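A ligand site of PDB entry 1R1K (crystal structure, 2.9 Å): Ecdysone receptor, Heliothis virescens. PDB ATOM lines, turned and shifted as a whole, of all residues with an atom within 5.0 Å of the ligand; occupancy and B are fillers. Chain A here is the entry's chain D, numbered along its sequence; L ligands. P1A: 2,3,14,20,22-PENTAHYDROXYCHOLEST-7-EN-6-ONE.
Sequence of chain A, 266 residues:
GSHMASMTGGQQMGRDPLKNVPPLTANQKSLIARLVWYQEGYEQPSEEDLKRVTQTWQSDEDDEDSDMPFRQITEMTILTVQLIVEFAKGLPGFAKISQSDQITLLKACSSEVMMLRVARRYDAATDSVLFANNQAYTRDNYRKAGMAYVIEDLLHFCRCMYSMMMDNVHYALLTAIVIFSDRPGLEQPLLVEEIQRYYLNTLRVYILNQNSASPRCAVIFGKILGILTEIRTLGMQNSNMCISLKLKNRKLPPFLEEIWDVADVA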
ATOM      1  N   TYR A  42     -15.285   7.597  14.541  1.00  0.00           N
ATOM      2  CA  TYR A  42     -16.579   7.433  13.896  1.00  0.00           C
ATOM      3  C   TYR A  42     -17.615   8.552  14.020  1.00  0.00           C
ATOM      4  O   TYR A  42     -18.711   8.377  13.539  1.00  0.00           O
ATOM      5  CB  TYR A  42     -17.228   6.129  14.355  1.00  0.00           C
ATOM      6  CG  TYR A  42     -16.484   4.875  13.939  1.00  0.00           C
ATOM      7  CD1 TYR A  42     -15.625   4.198  14.829  1.00  0.00           C
ATOM      8  CD2 TYR A  42     -16.657   4.337  12.653  1.00  0.00           C
ATOM      9  CE1 TYR A  42     -14.971   3.021  14.446  1.00  0.00           C
ATOM     10  CE2 TYR A  42     -16.005   3.151  12.264  1.00  0.00           C
ATOM     11  CZ  TYR A  42     -15.166   2.488  13.162  1.00  0.00           C
ATOM     12  OH  TYR A  42     -14.548   1.296  12.761  1.00  0.00           O
ATOM     13  N   GLU A  43     -17.304   9.694  14.630  1.00  0.00           N
ATOM     14  CA  GLU A  43     -18.342  10.723  14.757  1.00  0.00           C
ATOM     15  C   GLU A  43     -19.036  11.009  13.449  1.00  0.00           C
ATOM     16  O   GLU A  43     -20.258  11.160  13.442  1.00  0.00           O
ATOM     17  CB  GLU A  43     -17.823  12.053  15.342  1.00  0.00           C
ATOM     18  CG  GLU A  43     -18.946  13.057  15.728  1.00  0.00           C
ATOM     19  CD  GLU A  43     -19.841  12.604  16.929  1.00  0.00           C
ATOM     20  OE1 GLU A  43     -21.091  12.447  16.764  1.00  0.00           O
ATOM     21  OE2 GLU A  43     -19.289  12.393  18.050  1.00  0.00           O
ATOM     22  N   GLN A  44     -18.281  11.077  12.344  1.00  0.00           N
ATOM     23  CA  GLN A  44     -18.867  11.354  11.024  1.00  0.00           C
ATOM     24  C   GLN A  44     -18.578  10.281   9.995  1.00  0.00           C
ATOM     25  O   GLN A  44     -17.621   9.522  10.105  1.00  0.00           O
ATOM     26  CB  GLN A  44     -18.357  12.672  10.441  1.00  0.00           C
ATOM     27  CG  GLN A  44     -18.589  13.883  11.293  1.00  0.00           C
ATOM     28  CD  GLN A  44     -18.418  15.168  10.506  1.00  0.00           C
ATOM     29  OE1 GLN A  44     -18.769  16.258  10.977  1.00  0.00           O
ATOM     30  NE2 GLN A  44     -17.883  15.054   9.301  1.00  0.00           N
ATOM     31  N   PRO A  45     -19.424  10.193   8.965  1.00  0.00           N
ATOM     32  CA  PRO A  45     -19.203   9.185   7.926  1.00  0.00           C
ATOM     33  C   PRO A  45     -18.127   9.697   7.008  1.00  0.00           C
ATOM     34  O   PRO A  45     -18.038  10.903   6.781  1.00  0.00           O
ATOM     35  CB  PRO A  45     -20.567   9.107   7.241  1.00  0.00           C
ATOM     36  CG  PRO A  45     -21.077  10.477   7.389  1.00  0.00           C
ATOM     37  CD  PRO A  45     -20.765  10.779   8.824  1.00  0.00           C
ATOM     38  N   ILE A  73     -32.239  13.266   5.579  1.00  0.00           N
ATOM     39  CA  ILE A  73     -32.413  12.776   6.950  1.00  0.00           C
ATOM     40  C   ILE A  73     -32.359  11.254   6.996  1.00  0.00           C
ATOM     41  O   ILE A  73     -31.651  10.682   7.803  1.00  0.00           O
ATOM     42  CB  ILE A  73     -33.758  13.223   7.560  1.00  0.00           C
ATOM     43  CG1 ILE A  73     -33.805  14.743   7.687  1.00  0.00           C
ATOM     44  CG2 ILE A  73     -33.961  12.551   8.931  1.00  0.00           C
ATOM     45  CD1 ILE A  73     -35.053  15.233   8.358  1.00  0.00           C
ATOM     46  N   THR A  74     -33.112  10.587   6.150  1.00  0.00           N
ATOM     47  CA  THR A  74     -33.115   9.120   6.110  1.00  0.00           C
ATOM     48  C   THR A  74     -31.765   8.553   5.662  1.00  0.00           C
ATOM     49  O   THR A  74     -31.207   7.686   6.304  1.00  0.00           O
ATOM     50  CB  THR A  74     -34.241   8.617   5.184  1.00  0.00           C
ATOM     51  OG1 THR A  74     -34.181   9.330   3.936  1.00  0.00           O
ATOM     52  CG2 THR A  74     -35.604   8.840   5.832  1.00  0.00           C
ATOM     53  N   MET A  76     -28.754  10.007   5.761  1.00  0.00           N
ATOM     54  CA  MET A  76     -27.760  10.313   6.782  1.00  0.00           C
ATOM     55  C   MET A  76     -27.896   9.389   7.984  1.00  0.00           C
ATOM     56  O   MET A  76     -26.894   9.025   8.598  1.00  0.00           O
ATOM     57  CB  MET A  76     -27.901  11.744   7.261  1.00  0.00           C
ATOM     58  CG  MET A  76     -27.237  12.782   6.392  1.00  0.00           C
ATOM     59  SD  MET A  76     -25.509  12.379   6.112  1.00  0.00           S
ATOM     60  CE  MET A  76     -25.443  12.465   4.362  1.00  0.00           C
ATOM     61  N   THR A  77     -29.131   8.998   8.309  1.00  0.00           N
ATOM     62  CA  THR A  77     -29.368   8.098   9.430  1.00  0.00           C
ATOM     63  C   THR A  77     -28.768   6.736   9.149  1.00  0.00           C
ATOM     64  O   THR A  77     -28.206   6.102  10.062  1.00  0.00           O
ATOM     65  CB  THR A  77     -30.849   7.919   9.665  1.00  0.00           C
ATOM     66  OG1 THR A  77     -31.477   9.197   9.672  1.00  0.00           O
ATOM     67  CG2 THR A  77     -31.089   7.273  11.014  1.00  0.00           C
ATOM     68  N   THR A  80     -25.279   7.019   9.973  1.00  0.00           N
ATOM     69  CA  THR A  80     -25.095   7.090  11.409  1.00  0.00           C
ATOM     70  C   THR A  80     -25.105   5.685  12.002  1.00  0.00           C
ATOM     71  O   THR A  80     -24.184   5.289  12.691  1.00  0.00           O
ATOM     72  CB  THR A  80     -26.210   7.909  12.082  1.00  0.00           C
ATOM     73  OG1 THR A  80     -26.149   9.267  11.604  1.00  0.00           O
ATOM     74  CG2 THR A  80     -26.065   7.868  13.617  1.00  0.00           C
ATOM     75  N   LEU A  83     -21.980   3.591  11.387  1.00  0.00           N
ATOM     76  CA  LEU A  83     -20.886   4.036  12.248  1.00  0.00           C
ATOM     77  C   LEU A  83     -21.068   3.500  13.667  1.00  0.00           C
ATOM     78  O   LEU A  83     -20.121   2.979  14.292  1.00  0.00           O
ATOM     79  CB  LEU A  83     -20.847   5.574  12.298  1.00  0.00           C
ATOM     80  CG  LEU A  83     -20.168   6.486  11.266  1.00  0.00           C
ATOM     81  CD1 LEU A  83     -19.874   5.745   9.971  1.00  0.00           C
ATOM     82  CD2 LEU A  83     -21.066   7.720  11.057  1.00  0.00           C
ATOM     83  N   MET A 114     -27.676   6.694  18.690  1.00  0.00           N
ATOM     84  CA  MET A 114     -27.898   7.683  17.680  1.00  0.00           C
ATOM     85  C   MET A 114     -28.451   8.941  18.331  1.00  0.00           C
ATOM     86  O   MET A 114     -28.485  10.005  17.736  1.00  0.00           O
ATOM     87  CB  MET A 114     -28.907   7.131  16.687  1.00  0.00           C
ATOM     88  CG  MET A 114     -29.626   8.181  15.945  1.00  0.00           C
ATOM     89  SD  MET A 114     -30.754   7.392  14.890  1.00  0.00           S
ATOM     90  CE  MET A 114     -29.546   6.770  13.701  1.00  0.00           C
ATOM     91  N   MET A 115     -28.912   8.797  19.565  1.00  0.00           N
ATOM     92  CA  MET A 115     -29.511   9.877  20.339  1.00  0.00           C
ATOM     93  C   MET A 115     -28.407  10.707  21.033  1.00  0.00           C
ATOM     94  O   MET A 115     -28.455  11.950  21.104  1.00  0.00           O
ATOM     95  CB  MET A 115     -30.434   9.227  21.351  1.00  0.00           C
ATOM     96  CG  MET A 115     -31.911   9.498  21.173  1.00  0.00           C
ATOM     97  SD  MET A 115     -32.525  10.014  19.570  1.00  0.00           S
ATOM     98  CE  MET A 115     -33.504   8.623  19.197  1.00  0.00           C
ATOM     99  N   ARG A 117     -25.500  10.788  19.903  1.00  0.00           N
ATOM    100  CA  ARG A 117     -24.848  11.471  18.795  1.00  0.00           C
ATOM    101  C   ARG A 117     -25.618  12.669  18.218  1.00  0.00           C
ATOM    102  O   ARG A 117     -25.030  13.543  17.605  1.00  0.00           O
ATOM    103  CB  ARG A 117     -24.508  10.475  17.710  1.00  0.00           C
ATOM    104  CG  ARG A 117     -23.688   9.329  18.231  1.00  0.00           C
ATOM    105  CD  ARG A 117     -23.767   8.170  17.291  1.00  0.00           C
ATOM    106  NE  ARG A 117     -22.998   8.404  16.074  1.00  0.00           N
ATOM    107  CZ  ARG A 117     -21.904   7.706  15.767  1.00  0.00           C
ATOM    108  NH1 ARG A 117     -21.465   6.749  16.597  1.00  0.00           N
ATOM    109  NH2 ARG A 117     -21.270   7.969  14.633  1.00  0.00           N
ATOM    110  N   VAL A 118     -26.922  12.736  18.374  1.00  0.00           N
ATOM    111  CA  VAL A 118     -27.527  13.941  17.845  1.00  0.00           C
ATOM    112  C   VAL A 118     -27.278  15.064  18.890  1.00  0.00           C
ATOM    113  O   VAL A 118     -27.234  16.247  18.555  1.00  0.00           O
ATOM    114  CB  VAL A 118     -29.061  13.774  17.525  1.00  0.00           C
ATOM    115  CG1 VAL A 118     -29.857  13.629  18.787  1.00  0.00           C
ATOM    116  CG2 VAL A 118     -29.544  14.976  16.759  1.00  0.00           C
ATOM    117  N   ARG A 121     -24.063  17.082  18.203  1.00  0.00           N
ATOM    118  CA  ARG A 121     -24.048  18.018  17.085  1.00  0.00           C
ATOM    119  C   ARG A 121     -25.175  19.059  17.212  1.00  0.00           C
ATOM    120  O   ARG A 121     -25.616  19.666  16.219  1.00  0.00           O
ATOM    121  CB  ARG A 121     -24.187  17.296  15.724  1.00  0.00           C
ATOM    122  CG  ARG A 121     -23.195  16.172  15.449  1.00  0.00           C
ATOM    123  CD  ARG A 121     -21.738  16.618  15.486  1.00  0.00           C
ATOM    124  NE  ARG A 121     -21.328  17.441  14.333  1.00  0.00           N
ATOM    125  CZ  ARG A 121     -21.200  16.976  13.089  1.00  0.00           C
ATOM    126  NH1 ARG A 121     -21.452  15.693  12.824  1.00  0.00           N
ATOM    127  NH2 ARG A 121     -20.824  17.799  12.124  1.00  0.00           N
ATOM    128  N   VAL A 129     -30.034  21.076  14.688  1.00  0.00           N
ATOM    129  CA  VAL A 129     -29.063  19.976  14.702  1.00  0.00           C
ATOM    130  C   VAL A 129     -28.204  20.129  13.474  1.00  0.00           C
ATOM    131  O   VAL A 129     -28.711  20.455  12.405  1.00  0.00           O
ATOM    132  CB  VAL A 129     -29.698  18.595  14.616  1.00  0.00           C
ATOM    133  CG1 VAL A 129     -28.610  17.529  14.819  1.00  0.00           C
ATOM    134  CG2 VAL A 129     -30.784  18.435  15.664  1.00  0.00           C
ATOM    135  N   LEU A 130     -26.901  19.892  13.620  1.00  0.00           N
ATOM    136  CA  LEU A 130     -26.002  20.027  12.488  1.00  0.00           C
ATOM    137  C   LEU A 130     -25.566  18.713  11.873  1.00  0.00           C
ATOM    138  O   LEU A 130     -24.822  17.944  12.481  1.00  0.00           O
ATOM    139  CB  LEU A 130     -24.766  20.811  12.914  1.00  0.00           C
ATOM    140  CG  LEU A 130     -24.872  22.320  12.695  1.00  0.00           C
ATOM    141  CD1 LEU A 130     -24.081  23.018  13.780  1.00  0.00           C
ATOM    142  CD2 LEU A 130     -24.380  22.685  11.284  1.00  0.00           C
ATOM    143  N   PHE A 131     -26.022  18.464  10.648  1.00  0.00           N
ATOM    144  CA  PHE A 131     -25.664  17.234   9.948  1.00  0.00           C
ATOM    145  C   PHE A 131     -24.200  17.237   9.528  1.00  0.00           C
ATOM    146  O   PHE A 131     -23.611  18.292   9.381  1.00  0.00           O
ATOM    147  CB  PHE A 131     -26.548  17.028   8.711  1.00  0.00           C
ATOM    148  CG  PHE A 131     -27.954  16.597   9.019  1.00  0.00           C
ATOM    149  CD1 PHE A 131     -28.598  17.029  10.178  1.00  0.00           C
ATOM    150  CD2 PHE A 131     -28.666  15.807   8.134  1.00  0.00           C
ATOM    151  CE1 PHE A 131     -29.917  16.689  10.448  1.00  0.00           C
ATOM    152  CE2 PHE A 131     -29.998  15.455   8.389  1.00  0.00           C
ATOM    153  CZ  PHE A 131     -30.618  15.906   9.548  1.00  0.00           C
ATOM    154  N   ALA A 132     -23.651  16.051   9.320  1.00  0.00           N
ATOM    155  CA  ALA A 132     -22.252  15.842   8.954  1.00  0.00           C
ATOM    156  C   ALA A 132     -21.766  16.635   7.743  1.00  0.00           C
ATOM    157  O   ALA A 132     -20.564  16.706   7.487  1.00  0.00           O
ATOM    158  CB  ALA A 132     -21.998  14.348   8.727  1.00  0.00           C
ATOM    159  N   ASN A 133     -22.682  17.219   7.001  1.00  0.00           N
ATOM    160  CA  ASN A 133     -22.327  18.025   5.841  1.00  0.00           C
ATOM    161  C   ASN A 133     -22.349  19.497   6.251  1.00  0.00           C
ATOM    162  O   ASN A 133     -22.459  20.385   5.405  1.00  0.00           O
ATOM    163  CB  ASN A 133     -23.332  17.801   4.712  1.00  0.00           C
ATOM    164  CG  ASN A 133     -24.654  18.529   4.962  1.00  0.00           C
ATOM    165  OD1 ASN A 133     -25.202  18.520   6.080  1.00  0.00           O
ATOM    166  ND2 ASN A 133     -25.196  19.130   3.912  1.00  0.00           N
ATOM    167  N   TYR A 142     -37.474  19.413   9.998  1.00  0.00           N
ATOM    168  CA  TYR A 142     -38.010  18.139  10.390  1.00  0.00           C
ATOM    169  C   TYR A 142     -39.517  18.144  10.155  1.00  0.00           C
ATOM    170  O   TYR A 142     -40.124  17.088   9.960  1.00  0.00           O
ATOM    171  CB  TYR A 142     -37.689  17.846  11.854  1.00  0.00           C
ATOM    172  CG  TYR A 142     -36.346  17.188  12.076  1.00  0.00           C
ATOM    173  CD1 TYR A 142     -35.154  17.924  12.027  1.00  0.00           C
ATOM    174  CD2 TYR A 142     -36.257  15.818  12.319  1.00  0.00           C
ATOM    175  CE1 TYR A 142     -33.913  17.307  12.230  1.00  0.00           C
ATOM    176  CE2 TYR A 142     -35.026  15.198  12.514  1.00  0.00           C
ATOM    177  CZ  TYR A 142     -33.864  15.944  12.463  1.00  0.00           C
ATOM    178  OH  TYR A 142     -32.656  15.291  12.573  1.00  0.00           O
ATOM    179  N   MET A 147     -41.143  14.498   9.786  1.00  0.00           N
ATOM    180  CA  MET A 147     -40.554  13.999  11.027  1.00  0.00           C
ATOM    181  C   MET A 147     -40.986  14.966  12.153  1.00  0.00           C
ATOM    182  O   MET A 147     -40.437  14.927  13.247  1.00  0.00           O
ATOM    183  CB  MET A 147     -39.028  13.997  10.920  1.00  0.00           C
ATOM    184  CG  MET A 147     -38.479  13.414   9.657  1.00  0.00           C
ATOM    185  SD  MET A 147     -38.536  11.616   9.691  1.00  0.00           S
ATOM    186  CE  MET A 147     -36.875  11.179   9.152  1.00  0.00           C
ATOM    187  N   VAL A 150     -41.070  13.605  15.891  1.00  0.00           N
ATOM    188  CA  VAL A 150     -39.878  13.293  16.620  1.00  0.00           C
ATOM    189  C   VAL A 150     -39.031  14.499  17.107  1.00  0.00           C
ATOM    190  O   VAL A 150     -38.280  14.383  18.123  1.00  0.00           O
ATOM    191  CB  VAL A 150     -39.038  12.384  15.742  1.00  0.00           C
ATOM    192  CG1 VAL A 150     -37.649  12.909  15.592  1.00  0.00           C
ATOM    193  CG2 VAL A 150     -39.048  11.025  16.307  1.00  0.00           C
ATOM    194  N   LEU A 154     -36.808  15.539  20.721  1.00  0.00           N
ATOM    195  CA  LEU A 154     -35.394  15.274  20.426  1.00  0.00           C
ATOM    196  C   LEU A 154     -34.535  16.485  20.726  1.00  0.00           C
ATOM    197  O   LEU A 154     -33.387  16.371  21.218  1.00  0.00           O
ATOM    198  CB  LEU A 154     -35.236  14.905  18.951  1.00  0.00           C
ATOM    199  CG  LEU A 154     -33.881  14.286  18.677  1.00  0.00           C
ATOM    200  CD1 LEU A 154     -33.935  12.814  18.994  1.00  0.00           C
ATOM    201  CD2 LEU A 154     -33.500  14.482  17.246  1.00  0.00           C
ATOM    202  N   ASN A 238     -38.671   7.076  18.065  1.00  0.00           N
ATOM    203  CA  ASN A 238     -38.019   6.853  16.773  1.00  0.00           C
ATOM    204  C   ASN A 238     -38.787   5.715  16.073  1.00  0.00           C
ATOM    205  O   ASN A 238     -39.076   5.789  14.881  1.00  0.00           O
ATOM    206  CB  ASN A 238     -36.566   6.498  17.021  1.00  0.00           C
ATOM    207  CG  ASN A 238     -35.830   6.073  15.782  1.00  0.00           C
ATOM    208  OD1 ASN A 238     -35.651   6.835  14.838  1.00  0.00           O
ATOM    209  ND2 ASN A 238     -35.367   4.831  15.790  1.00  0.00           N
ATOM    210  N   MET A 241     -42.138   6.659  14.920  1.00  0.00           N
ATOM    211  CA  MET A 241     -41.954   7.490  13.740  1.00  0.00           C
ATOM    212  C   MET A 241     -41.758   6.574  12.549  1.00  0.00           C
ATOM    213  O   MET A 241     -42.285   6.831  11.495  1.00  0.00           O
ATOM    214  CB  MET A 241     -40.734   8.418  13.905  1.00  0.00           C
ATOM    215  CG  MET A 241     -40.522   9.430  12.761  1.00  0.00           C
ATOM    216  SD  MET A 241     -41.518  10.957  12.867  1.00  0.00           S
ATOM    217  CE  MET A 241     -42.958  10.490  11.805  1.00  0.00           C
ATOM    218  N   CYS A 242     -40.999   5.504  12.728  1.00  0.00           N
ATOM    219  CA  CYS A 242     -40.771   4.560  11.635  1.00  0.00           C
ATOM    220  C   CYS A 242     -42.131   3.983  11.303  1.00  0.00           C
ATOM    221  O   CYS A 242     -42.459   3.850  10.132  1.00  0.00           O
ATOM    222  CB  CYS A 242     -39.806   3.440  12.029  1.00  0.00           C
ATOM    223  SG  CYS A 242     -38.055   3.958  12.286  1.00  0.00           S
ATOM    224  N   LEU A 245     -44.591   6.141   9.580  1.00  0.00           N
ATOM    225  CA  LEU A 245     -43.994   6.505   8.304  1.00  0.00           C
ATOM    226  C   LEU A 245     -44.208   5.399   7.291  1.00  0.00           C
ATOM    227  O   LEU A 245     -44.410   5.652   6.097  1.00  0.00           O
ATOM    228  CB  LEU A 245     -42.500   6.802   8.443  1.00  0.00           C
ATOM    229  CG  LEU A 245     -42.169   8.178   9.021  1.00  0.00           C
ATOM    230  CD1 LEU A 245     -40.663   8.275   9.153  1.00  0.00           C
ATOM    231  CD2 LEU A 245     -42.700   9.284   8.145  1.00  0.00           C
ATOM    232  N   TRP A 260     -34.450  -1.772  13.099  1.00  0.00           N
ATOM    233  CA  TRP A 260     -35.310  -1.361  14.197  1.00  0.00           C
ATOM    234  C   TRP A 260     -36.598  -2.186  14.371  1.00  0.00           C
ATOM    235  O   TRP A 260     -37.517  -1.758  15.069  1.00  0.00           O
ATOM    236  CB  TRP A 260     -35.678   0.105  14.070  1.00  0.00           C
ATOM    237  CG  TRP A 260     -34.512   1.013  14.319  1.00  0.00           C
ATOM    238  CD1 TRP A 260     -33.463   0.770  15.148  1.00  0.00           C
ATOM    239  CD2 TRP A 260     -34.263   2.268  13.699  1.00  0.00           C
ATOM    240  NE1 TRP A 260     -32.572   1.795  15.081  1.00  0.00           N
ATOM    241  CE2 TRP A 260     -33.045   2.739  14.195  1.00  0.00           C
ATOM    242  CE3 TRP A 260     -34.973   3.041  12.775  1.00  0.00           C
ATOM    243  CZ2 TRP A 260     -32.493   3.968  13.789  1.00  0.00           C
ATOM    244  CZ3 TRP A 260     -34.428   4.258  12.370  1.00  0.00           C
ATOM    245  CH2 TRP A 260     -33.192   4.704  12.878  1.00  0.00           C
HETATM  246  C5  P1A L   1     -24.929  13.178  11.452  1.00  0.00           C
HETATM  247  C10 P1A L   1     -25.595  13.058  12.891  1.00  0.00           C
HETATM  248  C1  P1A L   1     -24.481  12.477  13.951  1.00  0.00           C
HETATM  249  C2  P1A L   1     -23.845  11.180  13.373  1.00  0.00           C
HETATM  250  C3  P1A L   1     -23.226  11.377  11.917  1.00  0.00           C
HETATM  251  C4  P1A L   1     -24.226  11.938  10.910  1.00  0.00           C
HETATM  252  C9  P1A L   1     -26.885  12.056  12.838  1.00  0.00           C
HETATM  253  C19 P1A L   1     -25.892  14.579  13.341  1.00  0.00           C
HETATM  254  C11 P1A L   1     -27.607  12.000  14.262  1.00  0.00           C
HETATM  255  C8  P1A L   1     -27.846  12.457  11.547  1.00  0.00           C
HETATM  256  C12 P1A L   1     -29.032  11.515  14.146  1.00  0.00           C
HETATM  257  C14 P1A L   1     -29.294  12.017  11.691  1.00  0.00           C
HETATM  258  C13 P1A L   1     -29.931  12.342  13.099  1.00  0.00           C
HETATM  259  C18 P1A L   1     -29.986  13.878  13.468  1.00  0.00           C
HETATM  260  C17 P1A L   1     -31.393  11.817  12.859  1.00  0.00           C
HETATM  261  O14 P1A L   1     -29.130  10.632  11.384  1.00  0.00           O
HETATM  262  C15 P1A L   1     -30.378  12.464  10.646  1.00  0.00           C
HETATM  263  C20 P1A L   1     -32.591  11.917  13.854  1.00  0.00           C
HETATM  264  C16 P1A L   1     -31.709  12.342  11.406  1.00  0.00           C
HETATM  265  C22 P1A L   1     -33.942  11.235  13.142  1.00  0.00           C
HETATM  266  O20 P1A L   1     -32.804  13.268  14.017  1.00  0.00           O
HETATM  267  C21 P1A L   1     -32.203  11.318  15.329  1.00  0.00           C
HETATM  268  C6  P1A L   1     -25.990  13.638  10.363  1.00  0.00           C
HETATM  269  C7  P1A L   1     -27.430  13.199  10.486  1.00  0.00           C
HETATM  270  O3  P1A L   1     -22.266  12.247  11.984  1.00  0.00           O
HETATM  271  O2  P1A L   1     -22.875  10.650  14.245  1.00  0.00           O
HETATM  272  O22 P1A L   1     -35.096  11.392  13.973  1.00  0.00           O
HETATM  273  C23 P1A L   1     -33.853   9.665  12.858  1.00  0.00           C
HETATM  274  C24 P1A L   1     -35.160   9.266  12.157  1.00  0.00           C
HETATM  275  C25 P1A L   1     -35.226   8.003  11.354  1.00  0.00           C
HETATM  276  C26 P1A L   1     -34.803   8.294   9.951  1.00  0.00           C
HETATM  277  C27 P1A L   1     -36.666   7.516  11.438  1.00  0.00           C
HETATM  278  O6  P1A L   1     -25.724  14.298   9.421  1.00  0.00           O
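O20 of the ligand sits at hydrogen-bond distance from OH of Tyr 142 (2.5 Å). The backbone carbonyl oxygen of Glu 43 sits at hydrogen-bond distance from an oxygen (O3) of the ligand (2.7 Å). An oxygen (O6) of the ligand is in hydrogen-bond range of the backbone NH (N) of Ala 132 (2.7 Å). The guanidinium group (NE) of Arg 117 sits at hydrogen-bond distance from an oxygen (O2) of the ligand. OG1 of Thr 80 sits close to O14 of the ligand (3.3 Å). O14 of the ligand sits close to N of Thr 77 (3.5 Å). The side-chain hydroxyl (OG1) of Thr 77 lies close to an oxygen (O14) of the ligand.
N of Met 147 sits at hydrogen-bond distance from O of Tyr 142 (2.8 Å). The backbone carbonyl oxygen (O) of Tyr 42 sits at hydrogen-bond distance from the guanidinium group (NH2) of Arg 117 (2.8 Å). OG1 of Thr 80 sits at hydrogen-bond distance from O of Met 76 (3.1 Å). The backbone carbonyl oxygen (O) of Asn 238 is in hydrogen-bond range of the side-chain sulfur (SG) of Cys 242, at 3.3 Å. The backbone NH (N) of Leu 130 is in hydrogen-bond range of the backbone carbonyl oxygen (O) of Arg 121, at 2.9 Å. The guanidinium group (NH2) of Arg 121 is in hydrogen-bond range of the side-chain amide oxygen (OE1) of Gln 44 (2.8 Å).
CA of Gln 44 touches O3 of the ligand, at 3.6 Å. CD of Pro 45 touches O3 of the ligand, 3.8 Å away. Ile 73 touches the ligand. Met 76 touches the ligand. Met 114 touches the ligand. Val 118 touches the ligand. Arg 121 touches the ligand. Leu 130 touches the ligand. Phe 131 touches the ligand. Met 147 touches the ligand (CE to C26, 3.6 Å). Val 150 touches the ligand (CG1 to O22, 3.4 Å). Leu 154 touches the ligand (CD2 to O20, 3.5 Å). Asn 238 touches the ligand. SG of Cys 242 touches C27 of the ligand, 3.9 Å away. Trp 260 touches the ligand (CZ3 to C25, 3.96 Å). Hydrophobic or aromatic side chains within 4 Å of the ligand: Pro 45, Ile 73, Met 76, Met 114, Val 118, Phe 131, Ala 132, Tyr 142, Met 147, Val 150, Leu 154 and Trp 260. 21 residues have an atom within 4 Å of the ligand: Glu 43, Gln 44, Pro 45, Ile 73, Met 76, Thr 77, Thr 80, Met 114, Arg 117, Val 118, Arg 121, Leu 130, Phe 131, Ala 132, Tyr 142, Met 147, Val 150, Leu 154, Asn 238, Cys 242 and Trp 260.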
